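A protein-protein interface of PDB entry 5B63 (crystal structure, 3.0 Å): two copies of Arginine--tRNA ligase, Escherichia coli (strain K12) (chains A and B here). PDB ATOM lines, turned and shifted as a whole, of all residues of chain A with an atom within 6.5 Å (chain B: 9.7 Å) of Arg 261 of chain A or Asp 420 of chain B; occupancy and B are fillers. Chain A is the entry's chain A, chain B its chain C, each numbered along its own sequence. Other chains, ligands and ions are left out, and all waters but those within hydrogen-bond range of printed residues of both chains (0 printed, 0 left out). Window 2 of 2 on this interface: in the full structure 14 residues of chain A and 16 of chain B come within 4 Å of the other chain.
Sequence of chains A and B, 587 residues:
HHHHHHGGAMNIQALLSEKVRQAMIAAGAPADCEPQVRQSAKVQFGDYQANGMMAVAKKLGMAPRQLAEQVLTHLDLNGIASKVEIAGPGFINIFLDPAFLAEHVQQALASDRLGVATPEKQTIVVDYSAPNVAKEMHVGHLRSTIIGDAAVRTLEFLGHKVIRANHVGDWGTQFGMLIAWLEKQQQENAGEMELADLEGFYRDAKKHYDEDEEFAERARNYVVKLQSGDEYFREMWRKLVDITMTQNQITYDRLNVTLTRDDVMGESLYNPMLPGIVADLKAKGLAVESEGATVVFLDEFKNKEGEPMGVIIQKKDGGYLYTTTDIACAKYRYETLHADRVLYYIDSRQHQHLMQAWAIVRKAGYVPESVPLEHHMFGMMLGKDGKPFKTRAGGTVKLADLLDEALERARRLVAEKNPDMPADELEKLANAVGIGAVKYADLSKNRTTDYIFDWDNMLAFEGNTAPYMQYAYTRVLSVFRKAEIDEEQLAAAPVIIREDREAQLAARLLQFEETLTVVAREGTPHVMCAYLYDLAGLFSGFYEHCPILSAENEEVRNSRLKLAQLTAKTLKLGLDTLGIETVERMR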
ATOM      1  N   ASP A 242     -19.634  31.641 -32.877  1.00  0.00           N
ATOM      2  CA  ASP A 242     -20.687  30.805 -32.308  1.00  0.00           C
ATOM      3  C   ASP A 242     -20.369  30.317 -30.897  1.00  0.00           C
ATOM      4  O   ASP A 242     -21.276  30.055 -30.110  1.00  0.00           O
ATOM      5  CB  ASP A 242     -20.987  29.615 -33.221  1.00  0.00           C
ATOM      6  CG  ASP A 242     -21.611  30.035 -34.537  1.00  0.00           C
ATOM      7  OD1 ASP A 242     -21.448  31.210 -34.927  1.00  0.00           O
ATOM      8  OD2 ASP A 242     -22.263  29.189 -35.184  1.00  0.00           O
ATOM      9  N   MET A 245     -21.106  33.350 -28.573  1.00  0.00           N
ATOM     10  CA  MET A 245     -22.544  33.555 -28.452  1.00  0.00           C
ATOM     11  C   MET A 245     -23.244  32.398 -27.748  1.00  0.00           C
ATOM     12  O   MET A 245     -24.413  32.504 -27.380  1.00  0.00           O
ATOM     13  CB  MET A 245     -23.169  33.801 -29.827  1.00  0.00           C
ATOM     14  CG  MET A 245     -22.665  35.063 -30.513  1.00  0.00           C
ATOM     15  SD  MET A 245     -22.719  36.505 -29.432  1.00  0.00           S
ATOM     16  CE  MET A 245     -24.464  36.589 -29.058  1.00  0.00           C
ATOM     17  N   THR A 246     -22.531  31.290 -27.575  1.00  0.00           N
ATOM     18  CA  THR A 246     -23.067  30.161 -26.828  1.00  0.00           C
ATOM     19  C   THR A 246     -22.788  30.372 -25.346  1.00  0.00           C
ATOM     20  O   THR A 246     -23.621  30.068 -24.493  1.00  0.00           O
ATOM     21  CB  THR A 246     -22.458  28.826 -27.291  1.00  0.00           C
ATOM     22  OG1 THR A 246     -22.790  28.601 -28.667  1.00  0.00           O
ATOM     23  CG2 THR A 246     -22.994  27.673 -26.456  1.00  0.00           C
ATOM     24  N   GLN A 247     -21.607  30.905 -25.049  1.00  0.00           N
ATOM     25  CA  GLN A 247     -21.254  31.277 -23.687  1.00  0.00           C
ATOM     26  C   GLN A 247     -22.178  32.379 -23.187  1.00  0.00           C
ATOM     27  O   GLN A 247     -22.528  32.425 -22.008  1.00  0.00           O
ATOM     28  CB  GLN A 247     -19.804  31.758 -23.632  1.00  0.00           C
ATOM     29  CG  GLN A 247     -19.381  32.305 -22.280  1.00  0.00           C
ATOM     30  CD  GLN A 247     -19.190  31.216 -21.248  1.00  0.00           C
ATOM     31  OE1 GLN A 247     -18.440  30.264 -21.467  1.00  0.00           O
ATOM     32  NE2 GLN A 247     -19.868  31.347 -20.115  1.00  0.00           N
ATOM     33  N   GLN A 249     -25.316  33.070 -24.414  1.00  0.00           N
ATOM     34  CA  GLN A 249     -26.703  32.633 -24.342  1.00  0.00           C
ATOM     35  C   GLN A 249     -26.955  32.008 -22.981  1.00  0.00           C
ATOM     36  O   GLN A 249     -28.064  32.068 -22.452  1.00  0.00           O
ATOM     37  CB  GLN A 249     -27.024  31.631 -25.447  1.00  0.00           C
ATOM     38  CG  GLN A 249     -28.500  31.282 -25.528  1.00  0.00           C
ATOM     39  CD  GLN A 249     -29.365  32.485 -25.853  1.00  0.00           C
ATOM     40  OE1 GLN A 249     -28.977  33.351 -26.638  1.00  0.00           O
ATOM     41  NE2 GLN A 249     -30.539  32.552 -25.239  1.00  0.00           N
ATOM     42  N   ASP A 253     -29.676  33.288 -20.373  1.00  0.00           N
ATOM     43  CA  ASP A 253     -30.602  32.341 -19.762  1.00  0.00           C
ATOM     44  C   ASP A 253     -30.566  32.445 -18.245  1.00  0.00           C
ATOM     45  O   ASP A 253     -31.586  32.286 -17.572  1.00  0.00           O
ATOM     46  CB  ASP A 253     -30.257  30.917 -20.196  1.00  0.00           C
ATOM     47  CG  ASP A 253     -30.589  30.658 -21.651  1.00  0.00           C
ATOM     48  OD1 ASP A 253     -30.836  31.637 -22.387  1.00  0.00           O
ATOM     49  OD2 ASP A 253     -30.598  29.478 -22.060  1.00  0.00           O
ATOM     50  N   LEU A 259     -33.273  37.369 -25.097  1.00  0.00           N
ATOM     51  CA  LEU A 259     -32.452  37.330 -26.301  1.00  0.00           C
ATOM     52  C   LEU A 259     -32.210  35.907 -26.778  1.00  0.00           C
ATOM     53  O   LEU A 259     -32.288  34.959 -26.001  1.00  0.00           O
ATOM     54  CB  LEU A 259     -31.119  38.043 -26.072  1.00  0.00           C
ATOM     55  CG  LEU A 259     -31.146  39.557 -26.270  1.00  0.00           C
ATOM     56  CD1 LEU A 259     -29.827  40.153 -25.847  1.00  0.00           C
ATOM     57  CD2 LEU A 259     -31.437  39.888 -27.720  1.00  0.00           C
ATOM     58  N   THR A 260     -31.910  35.772 -28.065  1.00  0.00           N
ATOM     59  CA  THR A 260     -31.690  34.466 -28.663  1.00  0.00           C
ATOM     60  C   THR A 260     -30.558  34.552 -29.683  1.00  0.00           C
ATOM     61  O   THR A 260     -30.060  35.638 -29.971  1.00  0.00           O
ATOM     62  CB  THR A 260     -32.969  33.963 -29.351  1.00  0.00           C
ATOM     63  OG1 THR A 260     -34.115  34.527 -28.699  1.00  0.00           O
ATOM     64  CG2 THR A 260     -33.052  32.448 -29.281  1.00  0.00           C
ATOM     65  N   ARG A 261     -30.144  33.407 -30.215  1.00  0.00           N
ATOM     66  CA  ARG A 261     -29.115  33.377 -31.247  1.00  0.00           C
ATOM     67  C   ARG A 261     -29.623  34.011 -32.532  1.00  0.00           C
ATOM     68  O   ARG A 261     -28.938  34.832 -33.139  1.00  0.00           O
ATOM     69  CB  ARG A 261     -28.642  31.949 -31.517  1.00  0.00           C
ATOM     70  CG  ARG A 261     -27.692  31.403 -30.474  1.00  0.00           C
ATOM     71  CD  ARG A 261     -28.366  30.360 -29.607  1.00  0.00           C
ATOM     72  NE  ARG A 261     -27.414  29.684 -28.734  1.00  0.00           N
ATOM     73  CZ  ARG A 261     -26.625  28.686 -29.122  1.00  0.00           C
ATOM     74  NH1 ARG A 261     -26.671  28.251 -30.374  1.00  0.00           N
ATOM     75  NH2 ARG A 261     -25.788  28.127 -28.259  1.00  0.00           N
ATOM     76  N   ASP A 262     -30.829  33.635 -32.946  1.00  0.00           N
ATOM     77  CA  ASP A 262     -31.438  34.244 -34.126  1.00  0.00           C
ATOM     78  C   ASP A 262     -32.025  35.619 -33.817  1.00  0.00           C
ATOM     79  O   ASP A 262     -33.127  35.955 -34.245  1.00  0.00           O
ATOM     80  CB  ASP A 262     -32.485  33.324 -34.759  1.00  0.00           C
ATOM     81  CG  ASP A 262     -33.359  32.635 -33.733  1.00  0.00           C
ATOM     82  OD1 ASP A 262     -33.409  33.101 -32.575  1.00  0.00           O
ATOM     83  OD2 ASP A 262     -33.999  31.624 -34.090  1.00  0.00           O
ATOM     84  N   ASP A 263     -31.267  36.396 -33.051  1.00  0.00           N
ATOM     85  CA  ASP A 263     -31.564  37.795 -32.793  1.00  0.00           C
ATOM     86  C   ASP A 263     -30.277  38.575 -33.015  1.00  0.00           C
ATOM     87  O   ASP A 263     -30.208  39.778 -32.767  1.00  0.00           O
ATOM     88  CB  ASP A 263     -32.060  37.989 -31.362  1.00  0.00           C
ATOM     89  CG  ASP A 263     -33.523  37.626 -31.196  1.00  0.00           C
ATOM     90  OD1 ASP A 263     -34.283  37.761 -32.179  1.00  0.00           O
ATOM     91  OD2 ASP A 263     -33.915  37.212 -30.084  1.00  0.00           O
ATOM     92  N   VAL A 264     -29.257  37.867 -33.487  1.00  0.00           N
ATOM     93  CA  VAL A 264     -27.944  38.454 -33.711  1.00  0.00           C
ATOM     94  C   VAL A 264     -27.834  39.089 -35.093  1.00  0.00           C
ATOM     95  O   VAL A 264     -27.995  38.419 -36.113  1.00  0.00           O
ATOM     96  CB  VAL A 264     -26.829  37.407 -33.550  1.00  0.00           C
ATOM     97  CG1 VAL A 264     -25.515  37.944 -34.087  1.00  0.00           C
ATOM     98  CG2 VAL A 264     -26.693  37.002 -32.092  1.00  0.00           C
ATOM     99  N   MET A 265     -27.561  40.388 -35.111  1.00  0.00           N
ATOM    100  CA  MET A 265     -27.376  41.130 -36.350  1.00  0.00           C
ATOM    101  C   MET A 265     -26.219  42.100 -36.172  1.00  0.00           C
ATOM    102  O   MET A 265     -26.415  43.311 -36.130  1.00  0.00           O
ATOM    103  CB  MET A 265     -28.651  41.892 -36.703  1.00  0.00           C
ATOM    104  CG  MET A 265     -29.805  41.001 -37.121  1.00  0.00           C
ATOM    105  SD  MET A 265     -31.403  41.731 -36.736  1.00  0.00           S
ATOM    106  CE  MET A 265     -31.195  43.350 -37.457  1.00  0.00           C
ATOM    107  N   ARG B 411     -22.881  24.172 -16.875  1.00  0.00           N
ATOM    108  CA  ARG B 411     -23.754  24.947 -17.745  1.00  0.00           C
ATOM    109  C   ARG B 411     -23.252  24.893 -19.178  1.00  0.00           C
ATOM    110  O   ARG B 411     -24.024  24.667 -20.109  1.00  0.00           O
ATOM    111  CB  ARG B 411     -23.837  26.400 -17.275  1.00  0.00           C
ATOM    112  CG  ARG B 411     -24.657  26.610 -16.020  1.00  0.00           C
ATOM    113  CD  ARG B 411     -24.651  28.072 -15.614  1.00  0.00           C
ATOM    114  NE  ARG B 411     -25.412  28.309 -14.393  1.00  0.00           N
ATOM    115  CZ  ARG B 411     -24.870  28.650 -13.230  1.00  0.00           C
ATOM    116  NH1 ARG B 411     -23.556  28.807 -13.129  1.00  0.00           N
ATOM    117  NH2 ARG B 411     -25.641  28.844 -12.170  1.00  0.00           N
ATOM    118  N   ARG B 412     -21.949  25.091 -19.344  1.00  0.00           N
ATOM    119  CA  ARG B 412     -21.327  25.009 -20.655  1.00  0.00           C
ATOM    120  C   ARG B 412     -21.454  23.600 -21.213  1.00  0.00           C
ATOM    121  O   ARG B 412     -21.660  23.411 -22.412  1.00  0.00           O
ATOM    122  CB  ARG B 412     -19.852  25.381 -20.565  1.00  0.00           C
ATOM    123  CG  ARG B 412     -19.578  26.659 -19.808  1.00  0.00           C
ATOM    124  CD  ARG B 412     -18.086  26.902 -19.726  1.00  0.00           C
ATOM    125  NE  ARG B 412     -17.731  27.869 -18.693  1.00  0.00           N
ATOM    126  CZ  ARG B 412     -17.047  28.984 -18.920  1.00  0.00           C
ATOM    127  NH1 ARG B 412     -16.642  29.273 -20.148  1.00  0.00           N
ATOM    128  NH2 ARG B 412     -16.764  29.805 -17.921  1.00  0.00           N
ATOM    129  N   VAL B 414     -23.805  21.309 -20.611  1.00  0.00           N
ATOM    130  CA  VAL B 414     -25.172  20.978 -21.003  1.00  0.00           C
ATOM    131  C   VAL B 414     -25.636  21.820 -22.186  1.00  0.00           C
ATOM    132  O   VAL B 414     -26.171  21.293 -23.163  1.00  0.00           O
ATOM    133  CB  VAL B 414     -26.158  21.161 -19.834  1.00  0.00           C
ATOM    134  CG1 VAL B 414     -27.583  20.887 -20.291  1.00  0.00           C
ATOM    135  CG2 VAL B 414     -25.782  20.247 -18.682  1.00  0.00           C
ATOM    136  N   ALA B 415     -25.424  23.129 -22.100  1.00  0.00           N
ATOM    137  CA  ALA B 415     -25.797  24.033 -23.181  1.00  0.00           C
ATOM    138  C   ALA B 415     -24.830  23.902 -24.354  1.00  0.00           C
ATOM    139  O   ALA B 415     -24.219  24.879 -24.784  1.00  0.00           O
ATOM    140  CB  ALA B 415     -25.843  25.467 -22.683  1.00  0.00           C
ATOM    141  N   GLU B 416     -24.700  22.682 -24.859  1.00  0.00           N
ATOM    142  CA  GLU B 416     -23.813  22.374 -25.969  1.00  0.00           C
ATOM    143  C   GLU B 416     -24.318  21.092 -26.610  1.00  0.00           C
ATOM    144  O   GLU B 416     -24.374  20.971 -27.833  1.00  0.00           O
ATOM    145  CB  GLU B 416     -22.382  22.176 -25.473  1.00  0.00           C
ATOM    146  CG  GLU B 416     -21.353  22.014 -26.585  1.00  0.00           C
ATOM    147  CD  GLU B 416     -20.731  23.332 -27.005  1.00  0.00           C
ATOM    148  OE1 GLU B 416     -20.174  24.033 -26.132  1.00  0.00           O
ATOM    149  OE2 GLU B 416     -20.798  23.669 -28.206  1.00  0.00           O
ATOM    150  N   LYS B 417     -24.685  20.135 -25.762  1.00  0.00           N
ATOM    151  CA  LYS B 417     -25.315  18.904 -26.214  1.00  0.00           C
ATOM    152  C   LYS B 417     -26.668  19.254 -26.811  1.00  0.00           C
ATOM    153  O   LYS B 417     -27.027  18.787 -27.891  1.00  0.00           O
ATOM    154  CB  LYS B 417     -25.497  17.940 -25.043  1.00  0.00           C
ATOM    155  CG  LYS B 417     -24.227  17.681 -24.248  1.00  0.00           C
ATOM    156  CD  LYS B 417     -23.184  16.967 -25.090  1.00  0.00           C
ATOM    157  CE  LYS B 417     -21.885  16.787 -24.322  1.00  0.00           C
ATOM    158  NZ  LYS B 417     -20.890  15.984 -25.084  1.00  0.00           N
ATOM    159  N   ASN B 418     -27.415  20.085 -26.092  1.00  0.00           N
ATOM    160  CA  ASN B 418     -28.690  20.590 -26.584  1.00  0.00           C
ATOM    161  C   ASN B 418     -28.909  22.055 -26.215  1.00  0.00           C
ATOM    162  O   ASN B 418     -29.599  22.364 -25.243  1.00  0.00           O
ATOM    163  CB  ASN B 418     -29.848  19.720 -26.087  1.00  0.00           C
ATOM    164  CG  ASN B 418     -29.834  19.531 -24.585  1.00  0.00           C
ATOM    165  OD1 ASN B 418     -28.807  19.723 -23.934  1.00  0.00           O
ATOM    166  ND2 ASN B 418     -30.976  19.151 -24.024  1.00  0.00           N
ATOM    167  N   PRO B 419     -28.307  22.967 -26.991  1.00  0.00           N
ATOM    168  CA  PRO B 419     -28.554  24.401 -26.823  1.00  0.00           C
ATOM    169  C   PRO B 419     -29.963  24.755 -27.287  1.00  0.00           C
ATOM    170  O   PRO B 419     -30.698  23.864 -27.717  1.00  0.00           O
ATOM    171  CB  PRO B 419     -27.512  25.043 -27.739  1.00  0.00           C
ATOM    172  CG  PRO B 419     -27.240  24.011 -28.776  1.00  0.00           C
ATOM    173  CD  PRO B 419     -27.329  22.696 -28.060  1.00  0.00           C
ATOM    174  N   ASP B 420     -30.327  26.031 -27.195  1.00  0.00           N
ATOM    175  CA  ASP B 420     -31.681  26.494 -27.509  1.00  0.00           C
ATOM    176  C   ASP B 420     -32.732  25.838 -26.613  1.00  0.00           C
ATOM    177  O   ASP B 420     -33.925  25.869 -26.915  1.00  0.00           O
ATOM    178  CB  ASP B 420     -32.024  26.273 -28.987  1.00  0.00           C
ATOM    179  CG  ASP B 420     -31.260  27.202 -29.906  1.00  0.00           C
ATOM    180  OD1 ASP B 420     -30.194  27.702 -29.492  1.00  0.00           O
ATOM    181  OD2 ASP B 420     -31.724  27.432 -31.042  1.00  0.00           O
ATOM    182  N   MET B 421     -32.280  25.247 -25.513  1.00  0.00           N
ATOM    183  CA  MET B 421     -33.177  24.619 -24.553  1.00  0.00           C
ATOM    184  C   MET B 421     -33.337  25.515 -23.328  1.00  0.00           C
ATOM    185  O   MET B 421     -32.343  26.012 -22.803  1.00  0.00           O
ATOM    186  CB  MET B 421     -32.661  23.229 -24.168  1.00  0.00           C
ATOM    187  CG  MET B 421     -32.867  22.187 -25.255  1.00  0.00           C
ATOM    188  SD  MET B 421     -33.244  20.551 -24.598  1.00  0.00           S
ATOM    189  CE  MET B 421     -33.617  19.660 -26.106  1.00  0.00           C
ATOM    190  N   PRO B 422     -34.590  25.690 -22.862  1.00  0.00           N
ATOM    191  CA  PRO B 422     -35.119  26.668 -21.902  1.00  0.00           C
ATOM    192  C   PRO B 422     -34.110  27.443 -21.054  1.00  0.00           C
ATOM    193  O   PRO B 422     -33.263  28.164 -21.582  1.00  0.00           O
ATOM    194  CB  PRO B 422     -35.994  25.797 -21.003  1.00  0.00           C
ATOM    195  CG  PRO B 422     -36.568  24.791 -21.954  1.00  0.00           C
ATOM    196  CD  PRO B 422     -35.587  24.630 -23.106  1.00  0.00           C
ATOM    197  N   ALA B 423     -34.240  27.312 -19.738  1.00  0.00           N
ATOM    198  CA  ALA B 423     -33.388  28.016 -18.791  1.00  0.00           C
ATOM    199  C   ALA B 423     -33.547  27.373 -17.423  1.00  0.00           C
ATOM    200  O   ALA B 423     -32.596  27.285 -16.647  1.00  0.00           O
ATOM    201  CB  ALA B 423     -33.760  29.484 -18.730  1.00  0.00           C
ATOM    202  N   GLU B 425     -34.723  24.115 -17.110  1.00  0.00           N
ATOM    203  CA  GLU B 425     -34.079  22.845 -17.410  1.00  0.00           C
ATOM    204  C   GLU B 425     -32.701  23.106 -18.004  1.00  0.00           C
ATOM    205  O   GLU B 425     -32.384  22.663 -19.106  1.00  0.00           O
ATOM    206  CB  GLU B 425     -34.919  22.021 -18.380  1.00  0.00           C
ATOM    207  CG  GLU B 425     -34.698  20.529 -18.239  1.00  0.00           C
ATOM    208  CD  GLU B 425     -34.772  19.801 -19.561  1.00  0.00           C
ATOM    209  OE1 GLU B 425     -34.065  20.211 -20.506  1.00  0.00           O
ATOM    210  OE2 GLU B 425     -35.536  18.819 -19.652  1.00  0.00           O
ATOM    211  N   LEU B 426     -31.894  23.847 -17.255  1.00  0.00           N
ATOM    212  CA  LEU B 426     -30.544  24.199 -17.647  1.00  0.00           C
ATOM    213  C   LEU B 426     -29.815  24.545 -16.364  1.00  0.00           C
ATOM    214  O   LEU B 426     -28.593  24.447 -16.279  1.00  0.00           O
ATOM    215  CB  LEU B 426     -30.553  25.407 -18.582  1.00  0.00           C
ATOM    216  CG  LEU B 426     -29.198  25.889 -19.103  1.00  0.00           C
ATOM    217  CD1 LEU B 426     -28.794  25.117 -20.349  1.00  0.00           C
ATOM    218  CD2 LEU B 426     -29.222  27.385 -19.371  1.00  0.00           C
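The side-chain hydroxyl (OG1) of Thr 246 of chain A is in hydrogen-bond range of the backbone carbonyl oxygen (O) of Asp 242 of chain A, 2.5 Å away.
The guanidinium group (NH2) of Arg 261 of chain A lies within hydrogen-bond range of the side-chain hydroxyl (OG1) of Thr 246 of chain A (3.1 Å).
The side-chain carboxylate of Asp 253 of chain A is in hydrogen-bond range of the side-chain amide nitrogen of Gln 249 of chain A, at 3.0 Å.
SD of Met 421 of chain B is in hydrogen-bond range of ND2 of Asn 418 of chain B, at 2.7 Å.
Of chain B, only Pro 419 and Asp 420 come within 4 Å of Arg 261 of chain A.
Of the printed residues of chain A, Asp 420 of chain B touches Arg 261.
Thr 246 of chain A touches just one residue of chain B: Ala 415 (3.5 Å).
No residue of chain B comes within 4 Å of Asp 262 of chain A.
No residue of chain B comes within 4 Å of Val 264 of chain A.
Of the printed residues of chain A, Ala 423 of chain B touches Asp 253.
Of the printed residues of chain A, Met 421 of chain B touches Asp 253.
Of the printed residues of chain A, Ala 415 of chain B touches Thr 246 (3.5 Å).
Of the printed residues of chain B, Gln 247 of chain A touches Arg 412 (2.4 Å).
Printed residues of chain A within 4 Å of Arg 412 of chain B: Gln 247 (2.4 Å).
The nearest residue of chain B that does not touch Arg 261 of chain A is Ala 415 of chain B (5.0 Å).
Along chain B the printed residues that touch a printed residue of chain A span positions 412 to 426.
Among the printed residues, 8 pairs touch across the chains.
No position is printed for both chains.
Thr 246 of chain A touches Ala 415 of chain B.
Asp 253 of chain A touches Met 421 of chain B.
O of Asp 253 of chain A touches CB of Ala 423 of chain B, 3.7 Å away.
Asp 253 of chain A touches Leu 426 of chain B (OD2 to CD2, 3.7 Å).
Arg 261 of chain A touches Pro 419 of chain B (NH2 to CB, 3.6 Å).
OE1 of Gln 247 of chain A lies within hydrogen-bond range of NH1 of Arg 412 of chain B, at 2.4 Å.
NE of Arg 261 of chain A lies within salt-bridge range of OD1 of Asp 420 of chain B, 3.5 Å away.
The backbone carbonyl oxygen (O) of Pro 422 of chain B sits close to the side-chain carboxylate (OD2) of Asp 253 of chain A, 3.0 Å away.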
